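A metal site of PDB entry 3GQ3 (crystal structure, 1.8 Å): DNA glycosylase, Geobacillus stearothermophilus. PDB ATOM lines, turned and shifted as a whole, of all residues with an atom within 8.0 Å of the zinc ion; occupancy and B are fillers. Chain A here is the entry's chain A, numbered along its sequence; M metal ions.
SG of Cys 252 sits close to N of Arg 254.
The side-chain amide oxygen (OE1) of Gln 256 sits at hydrogen-bond distance from the backbone NH (N) of Cys 252 (2.8 Å).
The side-chain sulfur (SG) of Cys 232 sits close to the backbone NH (N) of Arg 234.
The backbone carbonyl oxygen (O) of Thr 237 is in hydrogen-bond range of the backbone NH (N) of Cys 232, at 2.7 Å.
SG of Cys 235 lies close to OG1 of Thr 237 (3.1 Å).
Within 4 Å of the zinc ion: Cys 232, Cys 235, Cys 252 and Cys 255.
The zinc ion is bound by SG of Cys 252 (2.3 Å), SG of Cys 232 (2.3 Å), SG of Cys 255 (2.3 Å) and SG of Cys 235 (2.3 Å).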
ATOM      1  N   PHE A 181      -6.673  12.218   9.367  1.00  0.00           N
ATOM      2  CA  PHE A 181      -7.896  13.031   9.244  1.00  0.00           C
ATOM      3  C   PHE A 181      -9.155  12.163   9.233  1.00  0.00           C
ATOM      4  O   PHE A 181     -10.119  12.424   9.943  1.00  0.00           O
ATOM      5  CB  PHE A 181      -7.894  13.904   7.984  1.00  0.00           C
ATOM      6  CG  PHE A 181      -9.232  14.564   7.725  1.00  0.00           C
ATOM      7  CD1 PHE A 181      -9.604  15.725   8.400  1.00  0.00           C
ATOM      8  CD2 PHE A 181     -10.150  13.993   6.833  1.00  0.00           C
ATOM      9  CE1 PHE A 181     -10.831  16.305   8.171  1.00  0.00           C
ATOM     10  CE2 PHE A 181     -11.408  14.569   6.607  1.00  0.00           C
ATOM     11  CZ  PHE A 181     -11.755  15.741   7.294  1.00  0.00           C
ATOM     12  N   TYR A 223      -8.542  15.453   1.580  1.00  0.00           N
ATOM     13  CA  TYR A 223      -9.260  16.187   2.609  1.00  0.00           C
ATOM     14  C   TYR A 223      -8.400  17.279   3.244  1.00  0.00           C
ATOM     15  O   TYR A 223      -8.897  18.357   3.599  1.00  0.00           O
ATOM     16  CB  TYR A 223      -9.639  15.195   3.691  1.00  0.00           C
ATOM     17  CG  TYR A 223     -10.794  14.308   3.328  1.00  0.00           C
ATOM     18  CD1 TYR A 223     -10.598  12.925   3.092  1.00  0.00           C
ATOM     19  CD2 TYR A 223     -12.087  14.843   3.202  1.00  0.00           C
ATOM     20  CE1 TYR A 223     -11.677  12.111   2.763  1.00  0.00           C
ATOM     21  CE2 TYR A 223     -13.148  14.033   2.865  1.00  0.00           C
ATOM     22  CZ  TYR A 223     -12.942  12.679   2.642  1.00  0.00           C
ATOM     23  OH  TYR A 223     -14.025  11.903   2.323  1.00  0.00           O
ATOM     24  N   VAL A 224      -7.113  17.002   3.417  1.00  0.00           N
ATOM     25  CA  VAL A 224      -6.239  17.913   4.188  1.00  0.00           C
ATOM     26  C   VAL A 224      -4.900  18.241   3.497  1.00  0.00           C
ATOM     27  O   VAL A 224      -4.428  19.382   3.596  1.00  0.00           O
ATOM     28  CB  VAL A 224      -5.963  17.419   5.664  1.00  0.00           C
ATOM     29  CG1 VAL A 224      -7.256  17.472   6.505  1.00  0.00           C
ATOM     30  CG2 VAL A 224      -5.267  16.020   5.732  1.00  0.00           C
ATOM     31  N   PRO A 231     -11.251  25.472   3.402  1.00  0.00           N
ATOM     32  CA  PRO A 231     -12.208  24.855   4.319  1.00  0.00           C
ATOM     33  C   PRO A 231     -12.153  23.330   4.317  1.00  0.00           C
ATOM     34  O   PRO A 231     -12.007  22.693   3.264  1.00  0.00           O
ATOM     35  CB  PRO A 231     -13.556  25.323   3.762  1.00  0.00           C
ATOM     36  CG  PRO A 231     -13.232  26.569   2.990  1.00  0.00           C
ATOM     37  CD  PRO A 231     -11.963  26.176   2.316  1.00  0.00           C
ATOM     38  N   CYS A 232     -12.293  22.772   5.509  1.00  0.00           N
ATOM     39  CA  CYS A 232     -12.466  21.357   5.656  1.00  0.00           C
ATOM     40  C   CYS A 232     -13.710  20.935   4.891  1.00  0.00           C
ATOM     41  O   CYS A 232     -14.752  21.585   4.983  1.00  0.00           O
ATOM     42  CB  CYS A 232     -12.605  21.005   7.131  1.00  0.00           C
ATOM     43  SG  CYS A 232     -12.912  19.220   7.436  1.00  0.00           S
ATOM     44  N   LYS A 233     -13.580  19.832   4.133  1.00  0.00           N
ATOM     45  CA  LYS A 233     -14.663  19.304   3.321  1.00  0.00           C
ATOM     46  C   LYS A 233     -15.753  18.655   4.149  1.00  0.00           C
ATOM     47  O   LYS A 233     -16.876  18.414   3.646  1.00  0.00           O
ATOM     48  CB  LYS A 233     -14.110  18.294   2.280  1.00  0.00           C
ATOM     49  CG  LYS A 233     -13.184  18.936   1.259  1.00  0.00           C
ATOM     50  CD  LYS A 233     -12.615  17.931   0.280  1.00  0.00           C
ATOM     51  CE  LYS A 233     -11.807  18.640  -0.770  1.00  0.00           C
ATOM     52  NZ  LYS A 233     -11.124  17.692  -1.714  1.00  0.00           N
ATOM     53  N   ARG A 234     -15.452  18.385   5.421  1.00  0.00           N
ATOM     54  CA  ARG A 234     -16.441  17.780   6.322  1.00  0.00           C
ATOM     55  C   ARG A 234     -17.097  18.771   7.274  1.00  0.00           C
ATOM     56  O   ARG A 234     -18.266  18.611   7.609  1.00  0.00           O
ATOM     57  CB  ARG A 234     -15.835  16.622   7.114  1.00  0.00           C
ATOM     58  CG  ARG A 234     -15.346  15.445   6.240  1.00  0.00           C
ATOM     59  CD  ARG A 234     -16.333  14.292   6.237  1.00  0.00           C
ATOM     60  NE  ARG A 234     -15.854  13.120   5.494  1.00  0.00           N
ATOM     61  CZ  ARG A 234     -15.066  12.165   5.999  1.00  0.00           C
ATOM     62  NH1 ARG A 234     -14.623  12.217   7.258  1.00  0.00           N
ATOM     63  NH2 ARG A 234     -14.714  11.142   5.227  1.00  0.00           N
ATOM     64  N   CYS A 235     -16.353  19.768   7.752  1.00  0.00           N
ATOM     65  CA  CYS A 235     -16.923  20.691   8.760  1.00  0.00           C
ATOM     66  C   CYS A 235     -16.751  22.178   8.424  1.00  0.00           C
ATOM     67  O   CYS A 235     -17.313  23.025   9.138  1.00  0.00           O
ATOM     68  CB  CYS A 235     -16.318  20.436  10.145  1.00  0.00           C
ATOM     69  SG  CYS A 235     -14.610  21.056  10.299  1.00  0.00           S
ATOM     70  N   GLY A 236     -15.987  22.487   7.367  1.00  0.00           N
ATOM     71  CA  GLY A 236     -15.811  23.880   6.917  1.00  0.00           C
ATOM     72  C   GLY A 236     -14.730  24.687   7.619  1.00  0.00           C
ATOM     73  O   GLY A 236     -14.422  25.843   7.212  1.00  0.00           O
ATOM     74  N   THR A 237     -14.147  24.106   8.660  1.00  0.00           N
ATOM     75  CA  THR A 237     -13.056  24.751   9.425  1.00  0.00           C
ATOM     76  C   THR A 237     -11.802  24.824   8.562  1.00  0.00           C
ATOM     77  O   THR A 237     -11.489  23.846   7.876  1.00  0.00           O
ATOM     78  CB  THR A 237     -12.726  23.931  10.701  1.00  0.00           C
ATOM     79  OG1 THR A 237     -13.891  23.831  11.548  1.00  0.00           O
ATOM     80  CG2 THR A 237     -11.550  24.566  11.501  1.00  0.00           C
ATOM     81  N   PRO A 238     -11.072  25.972   8.591  1.00  0.00           N
ATOM     82  CA  PRO A 238      -9.865  26.005   7.777  1.00  0.00           C
ATOM     83  C   PRO A 238      -8.845  24.962   8.203  1.00  0.00           C
ATOM     84  O   PRO A 238      -8.549  24.807   9.400  1.00  0.00           O
ATOM     85  CB  PRO A 238      -9.285  27.406   8.003  1.00  0.00           C
ATOM     86  CG  PRO A 238     -10.417  28.220   8.528  1.00  0.00           C
ATOM     87  CD  PRO A 238     -11.355  27.275   9.240  1.00  0.00           C
ATOM     88  N   ILE A 239      -8.345  24.234   7.215  1.00  0.00           N
ATOM     89  CA  ILE A 239      -7.258  23.287   7.390  1.00  0.00           C
ATOM     90  C   ILE A 239      -6.001  24.044   7.811  1.00  0.00           C
ATOM     91  O   ILE A 239      -5.746  25.196   7.361  1.00  0.00           O
ATOM     92  CB  ILE A 239      -7.050  22.476   6.087  1.00  0.00           C
ATOM     93  CG1 ILE A 239      -8.375  21.753   5.707  1.00  0.00           C
ATOM     94  CG2 ILE A 239      -5.795  21.549   6.147  1.00  0.00           C
ATOM     95  CD1 ILE A 239      -9.012  20.969   6.872  1.00  0.00           C
ATOM     96  N   TYR A 251      -3.962  19.219   8.851  1.00  0.00           N
ATOM     97  CA  TYR A 251      -5.016  18.651   9.702  1.00  0.00           C
ATOM     98  C   TYR A 251      -6.170  19.618   9.884  1.00  0.00           C
ATOM     99  O   TYR A 251      -6.013  20.815   9.687  1.00  0.00           O
ATOM    100  CB  TYR A 251      -4.470  18.231  11.092  1.00  0.00           C
ATOM    101  CG  TYR A 251      -3.946  19.388  11.887  1.00  0.00           C
ATOM    102  CD1 TYR A 251      -4.760  20.036  12.809  1.00  0.00           C
ATOM    103  CD2 TYR A 251      -2.645  19.884  11.672  1.00  0.00           C
ATOM    104  CE1 TYR A 251      -4.319  21.159  13.501  1.00  0.00           C
ATOM    105  CE2 TYR A 251      -2.182  21.004  12.386  1.00  0.00           C
ATOM    106  CZ  TYR A 251      -3.037  21.619  13.300  1.00  0.00           C
ATOM    107  OH  TYR A 251      -2.618  22.718  14.032  1.00  0.00           O
ATOM    108  N   CYS A 252      -7.327  19.071  10.267  1.00  0.00           N
ATOM    109  CA  CYS A 252      -8.487  19.893  10.637  1.00  0.00           C
ATOM    110  C   CYS A 252      -8.567  19.924  12.142  1.00  0.00           C
ATOM    111  O   CYS A 252      -8.730  18.860  12.769  1.00  0.00           O
ATOM    112  CB  CYS A 252      -9.780  19.320  10.057  1.00  0.00           C
ATOM    113  SG  CYS A 252     -11.258  20.230  10.663  1.00  0.00           S
ATOM    114  N   PRO A 253      -8.451  21.132  12.730  1.00  0.00           N
ATOM    115  CA  PRO A 253      -8.404  21.206  14.169  1.00  0.00           C
ATOM    116  C   PRO A 253      -9.764  20.924  14.836  1.00  0.00           C
ATOM    117  O   PRO A 253      -9.822  20.827  16.051  1.00  0.00           O
ATOM    118  CB  PRO A 253      -7.936  22.645  14.437  1.00  0.00           C
ATOM    119  CG  PRO A 253      -8.447  23.442  13.247  1.00  0.00           C
ATOM    120  CD  PRO A 253      -8.302  22.459  12.086  1.00  0.00           C
ATOM    121  N   ARG A 254     -10.849  20.837  14.051  1.00  0.00           N
ATOM    122  CA  ARG A 254     -12.145  20.453  14.584  1.00  0.00           C
ATOM    123  C   ARG A 254     -12.418  18.953  14.467  1.00  0.00           C
ATOM    124  O   ARG A 254     -12.839  18.318  15.441  1.00  0.00           O
ATOM    125  CB  ARG A 254     -13.291  21.225  13.911  1.00  0.00           C
ATOM    126  CG  ARG A 254     -14.648  20.849  14.465  1.00  0.00           C
ATOM    127  CD  ARG A 254     -15.774  21.668  13.861  1.00  0.00           C
ATOM    128  NE  ARG A 254     -17.032  21.322  14.497  1.00  0.00           N
ATOM    129  CZ  ARG A 254     -18.183  21.918  14.245  1.00  0.00           C
ATOM    130  NH1 ARG A 254     -19.263  21.533  14.908  1.00  0.00           N
ATOM    131  NH2 ARG A 254     -18.226  22.925  13.355  1.00  0.00           N
ATOM    132  N   CYS A 255     -12.213  18.405  13.267  1.00  0.00           N
ATOM    133  CA  CYS A 255     -12.481  16.991  13.029  1.00  0.00           C
ATOM    134  C   CYS A 255     -11.494  16.083  13.752  1.00  0.00           C
ATOM    135  O   CYS A 255     -11.864  14.966  14.142  1.00  0.00           O
ATOM    136  CB  CYS A 255     -12.425  16.676  11.521  1.00  0.00           C
ATOM    137  SG  CYS A 255     -13.863  17.306  10.600  1.00  0.00           S
ATOM    138  N   GLN A 256     -10.255  16.531  13.922  1.00  0.00           N
ATOM    139  CA  GLN A 256      -9.235  15.677  14.571  1.00  0.00           C
ATOM    140  C   GLN A 256      -9.010  16.080  16.026  1.00  0.00           C
ATOM    141  O   GLN A 256      -8.977  17.268  16.344  1.00  0.00           O
ATOM    142  CB  GLN A 256      -7.919  15.736  13.788  1.00  0.00           C
ATOM    143  CG  GLN A 256      -8.077  15.102  12.410  1.00  0.00           C
ATOM    144  CD  GLN A 256      -6.964  15.430  11.467  1.00  0.00           C
ATOM    145  OE1 GLN A 256      -7.130  16.244  10.552  1.00  0.00           O
ATOM    146  NE2 GLN A 256      -5.824  14.754  11.628  1.00  0.00           N
HETATM  147 ZN    ZN M   1     -13.114  19.343   9.740  1.00  0.00          ZN
